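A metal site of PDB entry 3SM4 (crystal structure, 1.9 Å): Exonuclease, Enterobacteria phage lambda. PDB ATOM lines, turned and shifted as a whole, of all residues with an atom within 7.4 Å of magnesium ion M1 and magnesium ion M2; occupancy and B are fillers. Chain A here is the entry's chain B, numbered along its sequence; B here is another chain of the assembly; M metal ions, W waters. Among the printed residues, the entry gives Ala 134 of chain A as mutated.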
ATOM      1  N   TRP A  27       5.593 -21.844  11.825  1.00  0.00           N
ATOM      2  CA  TRP A  27       4.718 -22.320  10.750  1.00  0.00           C
ATOM      3  C   TRP A  27       3.792 -23.443  11.212  1.00  0.00           C
ATOM      4  O   TRP A  27       2.599 -23.421  10.904  1.00  0.00           O
ATOM      5  CB  TRP A  27       5.538 -22.780   9.538  1.00  0.00           C
ATOM      6  CG  TRP A  27       4.704 -23.299   8.398  1.00  0.00           C
ATOM      7  CD1 TRP A  27       3.996 -22.554   7.494  1.00  0.00           C
ATOM      8  CD2 TRP A  27       4.507 -24.678   8.036  1.00  0.00           C
ATOM      9  NE1 TRP A  27       3.360 -23.380   6.597  1.00  0.00           N
ATOM     10  CE2 TRP A  27       3.662 -24.688   6.900  1.00  0.00           C
ATOM     11  CE3 TRP A  27       4.951 -25.896   8.562  1.00  0.00           C
ATOM     12  CZ2 TRP A  27       3.254 -25.876   6.282  1.00  0.00           C
ATOM     13  CZ3 TRP A  27       4.550 -27.072   7.947  1.00  0.00           C
ATOM     14  CH2 TRP A  27       3.707 -27.051   6.815  1.00  0.00           C
ATOM     15  N   SER A  38      -3.929 -28.985   2.127  1.00  0.00           N
ATOM     16  CA  SER A  38      -3.507 -30.376   1.947  1.00  0.00           C
ATOM     17  C   SER A  38      -4.411 -31.393   2.657  1.00  0.00           C
ATOM     18  O   SER A  38      -4.259 -32.607   2.464  1.00  0.00           O
ATOM     19  CB  SER A  38      -2.051 -30.567   2.381  1.00  0.00           C
ATOM     20  OG  SER A  38      -1.918 -30.436   3.786  1.00  0.00           O
ATOM     21  N   GLY A  84       9.533 -36.465  -0.614  1.00  0.00           N
ATOM     22  CA  GLY A  84       8.819 -35.255  -1.040  1.00  0.00           C
ATOM     23  C   GLY A  84       9.458 -33.996  -0.478  1.00  0.00           C
ATOM     24  O   GLY A  84       9.595 -32.990  -1.177  1.00  0.00           O
ATOM     25  N   GLU A  88      11.669 -31.078  -3.100  1.00  0.00           N
ATOM     26  CA  GLU A  88      10.810 -29.921  -3.324  1.00  0.00           C
ATOM     27  C   GLU A  88      11.579 -28.729  -3.907  1.00  0.00           C
ATOM     28  O   GLU A  88      11.125 -28.114  -4.874  1.00  0.00           O
ATOM     29  CB  GLU A  88      10.103 -29.520  -2.027  1.00  0.00           C
ATOM     30  CG  GLU A  88       9.021 -28.473  -2.196  1.00  0.00           C
ATOM     31  CD  GLU A  88       8.304 -28.176  -0.900  1.00  0.00           C
ATOM     32  OE1 GLU A  88       7.367 -28.911  -0.549  1.00  0.00           O
ATOM     33  OE2 GLU A  88       8.687 -27.188  -0.243  1.00  0.00           O
ATOM     34  N   ARG A  92      11.128 -26.988  -7.689  1.00  0.00           N
ATOM     35  CA  ARG A  92      10.792 -25.586  -7.891  1.00  0.00           C
ATOM     36  C   ARG A  92      11.769 -24.899  -8.856  1.00  0.00           C
ATOM     37  O   ARG A  92      11.350 -24.235  -9.798  1.00  0.00           O
ATOM     38  CB  ARG A  92      10.731 -24.852  -6.545  1.00  0.00           C
ATOM     39  CG  ARG A  92      10.201 -23.421  -6.608  1.00  0.00           C
ATOM     40  CD  ARG A  92       9.677 -22.929  -5.243  1.00  0.00           C
ATOM     41  NE  ARG A  92      10.550 -23.343  -4.142  1.00  0.00           N
ATOM     42  CZ  ARG A  92      10.175 -24.106  -3.122  1.00  0.00           C
ATOM     43  NH1 ARG A  92       8.924 -24.519  -2.997  1.00  0.00           N
ATOM     44  NH2 ARG A  92      11.059 -24.424  -2.179  1.00  0.00           N
ATOM     45  N   SER A 120      -0.848 -23.292   2.396  1.00  0.00           N
ATOM     46  CA  SER A 120       0.594 -23.064   2.393  1.00  0.00           C
ATOM     47  C   SER A 120       1.145 -23.386   0.998  1.00  0.00           C
ATOM     48  O   SER A 120       1.616 -24.500   0.760  1.00  0.00           O
ATOM     49  CB  SER A 120       1.294 -23.924   3.454  1.00  0.00           C
ATOM     50  OG  SER A 120       0.695 -23.745   4.728  1.00  0.00           O
ATOM     51  N   PRO A 121       1.079 -22.422   0.069  1.00  0.00           N
ATOM     52  CA  PRO A 121       1.479 -22.714  -1.311  1.00  0.00           C
ATOM     53  C   PRO A 121       2.937 -23.157  -1.445  1.00  0.00           C
ATOM     54  O   PRO A 121       3.782 -22.746  -0.648  1.00  0.00           O
ATOM     55  CB  PRO A 121       1.259 -21.386  -2.050  1.00  0.00           C
ATOM     56  CG  PRO A 121       1.215 -20.349  -0.970  1.00  0.00           C
ATOM     57  CD  PRO A 121       0.614 -21.029   0.215  1.00  0.00           C
ATOM     58  N   ASP A 122       3.211 -24.002  -2.434  1.00  0.00           N
ATOM     59  CA  ASP A 122       4.591 -24.367  -2.768  1.00  0.00           C
ATOM     60  C   ASP A 122       5.332 -23.221  -3.458  1.00  0.00           C
ATOM     61  O   ASP A 122       6.560 -23.243  -3.593  1.00  0.00           O
ATOM     62  CB  ASP A 122       4.625 -25.633  -3.616  1.00  0.00           C
ATOM     63  CG  ASP A 122       4.445 -26.894  -2.791  1.00  0.00           C
ATOM     64  OD1 ASP A 122       4.569 -26.825  -1.541  1.00  0.00           O
ATOM     65  OD2 ASP A 122       4.187 -27.968  -3.383  1.00  0.00           O
ATOM     66  N   GLY A 123       4.567 -22.226  -3.917  1.00  0.00           N
ATOM     67  CA  GLY A 123       5.130 -21.007  -4.481  1.00  0.00           C
ATOM     68  C   GLY A 123       4.070 -20.095  -5.066  1.00  0.00           C
ATOM     69  O   GLY A 123       2.937 -20.521  -5.304  1.00  0.00           O
ATOM     70  N   LEU A 131       1.554 -22.062  -7.222  1.00  0.00           N
ATOM     71  CA  LEU A 131       2.276 -23.275  -7.628  1.00  0.00           C
ATOM     72  C   LEU A 131       2.213 -24.360  -6.561  1.00  0.00           C
ATOM     73  O   LEU A 131       2.458 -24.101  -5.372  1.00  0.00           O
ATOM     74  CB  LEU A 131       3.747 -22.946  -7.961  1.00  0.00           C
ATOM     75  CG  LEU A 131       4.753 -24.100  -8.131  1.00  0.00           C
ATOM     76  CD1 LEU A 131       4.497 -24.913  -9.388  1.00  0.00           C
ATOM     77  CD2 LEU A 131       6.176 -23.559  -8.116  1.00  0.00           C
ATOM     78  N   GLU A 132       1.869 -25.566  -7.012  1.00  0.00           N
ATOM     79  CA  GLU A 132       1.935 -26.765  -6.186  1.00  0.00           C
ATOM     80  C   GLU A 132       2.900 -27.749  -6.842  1.00  0.00           C
ATOM     81  O   GLU A 132       2.782 -28.042  -8.034  1.00  0.00           O
ATOM     82  CB  GLU A 132       0.531 -27.384  -6.054  1.00  0.00           C
ATOM     83  CG  GLU A 132       0.494 -28.738  -5.306  1.00  0.00           C
ATOM     84  CD  GLU A 132       1.075 -28.674  -3.905  1.00  0.00           C
ATOM     85  OE1 GLU A 132       0.889 -27.645  -3.221  1.00  0.00           O
ATOM     86  OE2 GLU A 132       1.710 -29.655  -3.487  1.00  0.00           O
ATOM     87  N   LEU A 133       3.876 -28.231  -6.061  1.00  0.00           N
ATOM     88  CA  LEU A 133       4.840 -29.227  -6.518  1.00  0.00           C
ATOM     89  C   LEU A 133       4.546 -30.573  -5.875  1.00  0.00           C
ATOM     90  O   LEU A 133       4.107 -30.635  -4.726  1.00  0.00           O
ATOM     91  CB  LEU A 133       6.275 -28.840  -6.130  1.00  0.00           C
ATOM     92  CG  LEU A 133       7.154 -27.726  -6.735  1.00  0.00           C
ATOM     93  CD1 LEU A 133       6.920 -27.489  -8.230  1.00  0.00           C
ATOM     94  CD2 LEU A 133       7.004 -26.444  -5.966  1.00  0.00           C
ATOM     95  N   ALA A 134       4.801 -31.649  -6.604  1.00  0.00           N
ATOM     96  CA  ALA A 134       4.793 -32.984  -6.014  1.00  0.00           C
ATOM     97  C   ALA A 134       5.982 -33.779  -6.528  1.00  0.00           C
ATOM     98  O   ALA A 134       6.315 -33.719  -7.712  1.00  0.00           O
ATOM     99  CB  ALA A 134       3.475 -33.705  -6.315  1.00  0.00           C
ATOM    100  N   CYS A 135       6.630 -34.495  -5.621  1.00  0.00           N
ATOM    101  CA  CYS A 135       7.735 -35.370  -5.969  1.00  0.00           C
ATOM    102  C   CYS A 135       7.366 -36.782  -5.535  1.00  0.00           C
ATOM    103  O   CYS A 135       7.720 -37.205  -4.427  1.00  0.00           O
ATOM    104  CB  CYS A 135       9.032 -34.892  -5.303  1.00  0.00           C
ATOM    105  SG  CYS A 135       9.475 -33.137  -5.600  1.00  0.00           S
ATOM    106  N   TYR A 157      -5.041 -33.862  -4.322  1.00  0.00           N
ATOM    107  CA  TYR A 157      -4.271 -32.751  -4.890  1.00  0.00           C
ATOM    108  C   TYR A 157      -5.188 -31.716  -5.555  1.00  0.00           C
ATOM    109  O   TYR A 157      -4.953 -30.510  -5.447  1.00  0.00           O
ATOM    110  CB  TYR A 157      -3.249 -33.250  -5.911  1.00  0.00           C
ATOM    111  CG  TYR A 157      -1.997 -33.886  -5.337  1.00  0.00           C
ATOM    112  CD1 TYR A 157      -1.298 -33.293  -4.289  1.00  0.00           C
ATOM    113  CD2 TYR A 157      -1.490 -35.072  -5.885  1.00  0.00           C
ATOM    114  CE1 TYR A 157      -0.137 -33.876  -3.761  1.00  0.00           C
ATOM    115  CE2 TYR A 157      -0.332 -35.655  -5.380  1.00  0.00           C
ATOM    116  CZ  TYR A 157       0.330 -35.060  -4.323  1.00  0.00           C
ATOM    117  OH  TYR A 157       1.477 -35.636  -3.820  1.00  0.00           O
ATOM    118  N   GLN A 160      -6.851 -29.791  -2.902  1.00  0.00           N
ATOM    119  CA  GLN A 160      -5.801 -28.925  -2.350  1.00  0.00           C
ATOM    120  C   GLN A 160      -5.553 -27.679  -3.206  1.00  0.00           C
ATOM    121  O   GLN A 160      -5.497 -26.556  -2.688  1.00  0.00           O
ATOM    122  CB  GLN A 160      -4.508 -29.723  -2.166  1.00  0.00           C
ATOM    123  CG  GLN A 160      -3.313 -28.917  -1.655  1.00  0.00           C
ATOM    124  CD  GLN A 160      -2.051 -29.752  -1.515  1.00  0.00           C
ATOM    125  OE1 GLN A 160      -1.993 -30.912  -1.935  1.00  0.00           O
ATOM    126  NE2 GLN A 160      -1.015 -29.165  -0.906  1.00  0.00           N
ATOM    127  N   PHE A 175       0.364 -27.064 -11.437  1.00  0.00           N
ATOM    128  CA  PHE A 175       0.582 -28.322 -10.735  1.00  0.00           C
ATOM    129  C   PHE A 175       1.692 -29.091 -11.442  1.00  0.00           C
ATOM    130  O   PHE A 175       1.512 -29.551 -12.573  1.00  0.00           O
ATOM    131  CB  PHE A 175      -0.688 -29.158 -10.639  1.00  0.00           C
ATOM    132  CG  PHE A 175      -0.502 -30.463  -9.908  1.00  0.00           C
ATOM    133  CD1 PHE A 175      -0.472 -31.669 -10.595  1.00  0.00           C
ATOM    134  CD2 PHE A 175      -0.332 -30.488  -8.513  1.00  0.00           C
ATOM    135  CE1 PHE A 175      -0.296 -32.883  -9.924  1.00  0.00           C
ATOM    136  CE2 PHE A 175      -0.161 -31.693  -7.833  1.00  0.00           C
ATOM    137  CZ  PHE A 175      -0.134 -32.900  -8.541  1.00  0.00           C
ATOM    138  N   ALA A 176       2.830 -29.209 -10.759  1.00  0.00           N
ATOM    139  CA  ALA A 176       4.023 -29.798 -11.320  1.00  0.00           C
ATOM    140  C   ALA A 176       4.425 -31.067 -10.579  1.00  0.00           C
ATOM    141  O   ALA A 176       4.279 -31.158  -9.356  1.00  0.00           O
ATOM    142  CB  ALA A 176       5.158 -28.787 -11.289  1.00  0.00           C
ATOM    143  OP3  DA B   1      -2.131 -27.909   4.410  1.00  0.00           O
ATOM    144  P    DA B   1      -1.310 -26.728   4.055  1.00  0.00           P
ATOM    145  OP1  DA B   1      -1.922 -26.063   2.891  1.00  0.00           O
ATOM    146  OP2  DA B   1      -1.096 -25.944   5.296  1.00  0.00           O
ATOM    147  O5'  DA B   1       0.107 -27.258   3.563  1.00  0.00           O
ATOM    148  C5'  DA B   1       0.925 -28.060   4.403  1.00  0.00           C
ATOM    149  C4'  DA B   1       2.088 -28.572   3.575  1.00  0.00           C
ATOM    150  O4'  DA B   1       3.099 -29.189   4.399  1.00  0.00           O
ATOM    151  C3'  DA B   1       1.745 -29.630   2.534  1.00  0.00           C
ATOM    152  O3'  DA B   1       2.665 -29.445   1.480  1.00  0.00           O
ATOM    153  C2'  DA B   1       1.948 -30.942   3.280  1.00  0.00           C
ATOM    154  C1'  DA B   1       3.078 -30.594   4.261  1.00  0.00           C
ATOM    155  N9   DA B   1       2.924 -31.087   5.629  1.00  0.00           N
ATOM    156  C8   DA B   1       1.775 -31.461   6.277  1.00  0.00           C
ATOM    157  N7   DA B   1       1.976 -31.836   7.517  1.00  0.00           N
ATOM    158  C5   DA B   1       3.340 -31.687   7.694  1.00  0.00           C
ATOM    159  C6   DA B   1       4.194 -31.911   8.793  1.00  0.00           C
ATOM    160  N6   DA B   1       3.781 -32.366   9.983  1.00  0.00           N
ATOM    161  N1   DA B   1       5.514 -31.667   8.635  1.00  0.00           N
ATOM    162  C2   DA B   1       5.957 -31.216   7.454  1.00  0.00           C
ATOM    163  N3   DA B   1       5.239 -30.963   6.350  1.00  0.00           N
ATOM    164  C4   DA B   1       3.932 -31.225   6.542  1.00  0.00           C
ATOM    165  P    DG B   2       2.631 -30.374   0.182  1.00  0.00           P
ATOM    166  OP1  DG B   2       3.391 -29.651  -0.863  1.00  0.00           O
ATOM    167  OP2  DG B   2       1.231 -30.775  -0.079  1.00  0.00           O
ATOM    168  O5'  DG B   2       3.481 -31.657   0.636  1.00  0.00           O
ATOM    169  C5'  DG B   2       4.895 -31.590   0.749  1.00  0.00           C
ATOM    170  C4'  DG B   2       5.487 -32.898   1.244  1.00  0.00           C
ATOM    171  O4'  DG B   2       5.231 -33.035   2.659  1.00  0.00           O
ATOM    172  C3'  DG B   2       4.875 -34.160   0.637  1.00  0.00           C
ATOM    173  O3'  DG B   2       5.591 -34.468  -0.555  1.00  0.00           O
ATOM    174  C2'  DG B   2       5.066 -35.211   1.727  1.00  0.00           C
ATOM    175  C1'  DG B   2       5.282 -34.397   3.002  1.00  0.00           C
ATOM    176  N9   DG B   2       4.286 -34.588   4.063  1.00  0.00           N
ATOM    177  C8   DG B   2       2.927 -34.521   3.957  1.00  0.00           C
ATOM    178  N7   DG B   2       2.308 -34.724   5.089  1.00  0.00           N
ATOM    179  C5   DG B   2       3.327 -34.931   6.011  1.00  0.00           C
ATOM    180  C6   DG B   2       3.280 -35.196   7.400  1.00  0.00           C
ATOM    181  O6   DG B   2       2.278 -35.304   8.117  1.00  0.00           O
ATOM    182  N1   DG B   2       4.555 -35.346   7.957  1.00  0.00           N
ATOM    183  C2   DG B   2       5.726 -35.243   7.254  1.00  0.00           C
ATOM    184  N2   DG B   2       6.874 -35.420   7.946  1.00  0.00           N
ATOM    185  N3   DG B   2       5.790 -34.994   5.953  1.00  0.00           N
ATOM    186  C4   DG B   2       4.561 -34.845   5.390  1.00  0.00           C
ATOM    187  P    DC B   3       4.807 -34.924  -1.874  1.00  0.00           P
ATOM    188  OP1  DC B   3       5.714 -34.752  -3.039  1.00  0.00           O
ATOM    189  OP2  DC B   3       3.471 -34.260  -1.883  1.00  0.00           O
ATOM    190  O5'  DC B   3       4.580 -36.478  -1.637  1.00  0.00           O
ATOM    191  C5'  DC B   3       5.645 -37.414  -1.802  1.00  0.00           C
ATOM    192  C4'  DC B   3       5.152 -38.841  -1.622  1.00  0.00           C
ATOM    193  O4'  DC B   3       4.613 -38.987  -0.291  1.00  0.00           O
ATOM    194  C3'  DC B   3       4.064 -39.293  -2.598  1.00  0.00           C
ATOM    195  O3'  DC B   3       4.423 -40.530  -3.220  1.00  0.00           O
ATOM    196  C2'  DC B   3       2.808 -39.415  -1.733  1.00  0.00           C
ATOM    197  C1'  DC B   3       3.405 -39.727  -0.368  1.00  0.00           C
ATOM    198  N1   DC B   3       2.547 -39.346   0.784  1.00  0.00           N
ATOM    199  C2   DC B   3       2.435 -40.207   1.883  1.00  0.00           C
ATOM    200  O2   DC B   3       3.066 -41.278   1.902  1.00  0.00           O
ATOM    201  N3   DC B   3       1.642 -39.853   2.927  1.00  0.00           N
ATOM    202  C4   DC B   3       0.983 -38.695   2.905  1.00  0.00           C
ATOM    203  N4   DC B   3       0.220 -38.407   3.964  1.00  0.00           N
ATOM    204  C5   DC B   3       1.068 -37.800   1.800  1.00  0.00           C
ATOM    205  C6   DC B   3       1.855 -38.155   0.775  1.00  0.00           C
HETATM  206 MG    MG M   1       3.734 -30.105  -2.823  1.00  0.00          MG
HETATM  207 MG    MG M   2       3.807 -27.565   0.240  1.00  0.00          MG
HETATM  208  O   HOH W   1       3.646 -26.126   1.567  1.00  0.00           O
HETATM  209  O   HOH W   2       5.632 -27.897   1.376  1.00  0.00           O
HETATM  210  O   HOH W   3       2.938 -31.915  -2.562  1.00  0.00           O
HETATM  211  O   HOH W   4       5.880 -30.210  -2.345  1.00  0.00           O
HETATM  212  O   HOH W   5       1.710 -27.314  -0.559  1.00  0.00           O
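OP2 of DG 2 of chain B sits at hydrogen-bond distance from the side-chain amide nitrogen (NE2) of Gln 160, at 2.9 Å.
The side-chain hydroxyl (OG) of Ser 120 sits at hydrogen-bond distance from the indole nitrogen (NE1) of Trp 27 (3.3 Å).
NH1 of Arg 92 sits at hydrogen-bond distance from O of Asp 122, 2.8 Å away.
NH1 of Arg 92 lies within salt-bridge range of OE2 of Glu 88 (3.8 Å).
The backbone NH (N) of Asp 122 is in hydrogen-bond range of the backbone carbonyl oxygen (O) of Leu 131, 3.0 Å away.
The side-chain carboxylate (OE1) of Glu 132 sits at hydrogen-bond distance from the side-chain amide nitrogen (NE2) of Gln 160 (3.4 Å).
OP2 of DA 1 of chain B lies within hydrogen-bond range of the side-chain hydroxyl (OG) of Ser 120 (2.9 Å).
O of Glu 132 is in hydrogen-bond range of N of Ala 176 (3.0 Å).
Of the 21 residues printed, 4 come within 4 Å of magnesium ion M1.
The nearest printed residue that does not touch magnesium ion M1 is Ala 134 (4.2 Å).
Residues that only touch magnesium ion M2: Glu 88 and Ser 120.
Water W3 is bound to magnesium ion M1 (2.0 Å).
O of Leu 133 binds magnesium ion M1, at 2.0 Å.
OP1 of DG 2 of chain B is bound to magnesium ion M1 (2.0 Å).
OE2 of Glu 132 binds magnesium ion M1, 2.2 Å away.
Water W4 binds magnesium ion M1 (2.2 Å).
The side-chain carboxylate (OD2) of Asp 122 binds magnesium ion M1, 2.3 Å away.
Magnesium ion M1 has six donor atoms within binding distance.
Magnesium ion M2 is bound by water W1 (2.0 Å), OD1 of Asp 122 (2.1 Å), water W2 (2.2 Å), water W5 (2.3 Å), OP1 of DG 2 of chain B (2.4 Å) and O3' of DA 1 of chain B (2.5 Å).
Magnesium ion M2 has six donor atoms within binding distance.
Water W5 lies within hydrogen-bond range of OE1 of Glu 132 (2.8 Å), O of Ser 120 (3.1 Å) and NE2 of Gln 160 (3.3 Å).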
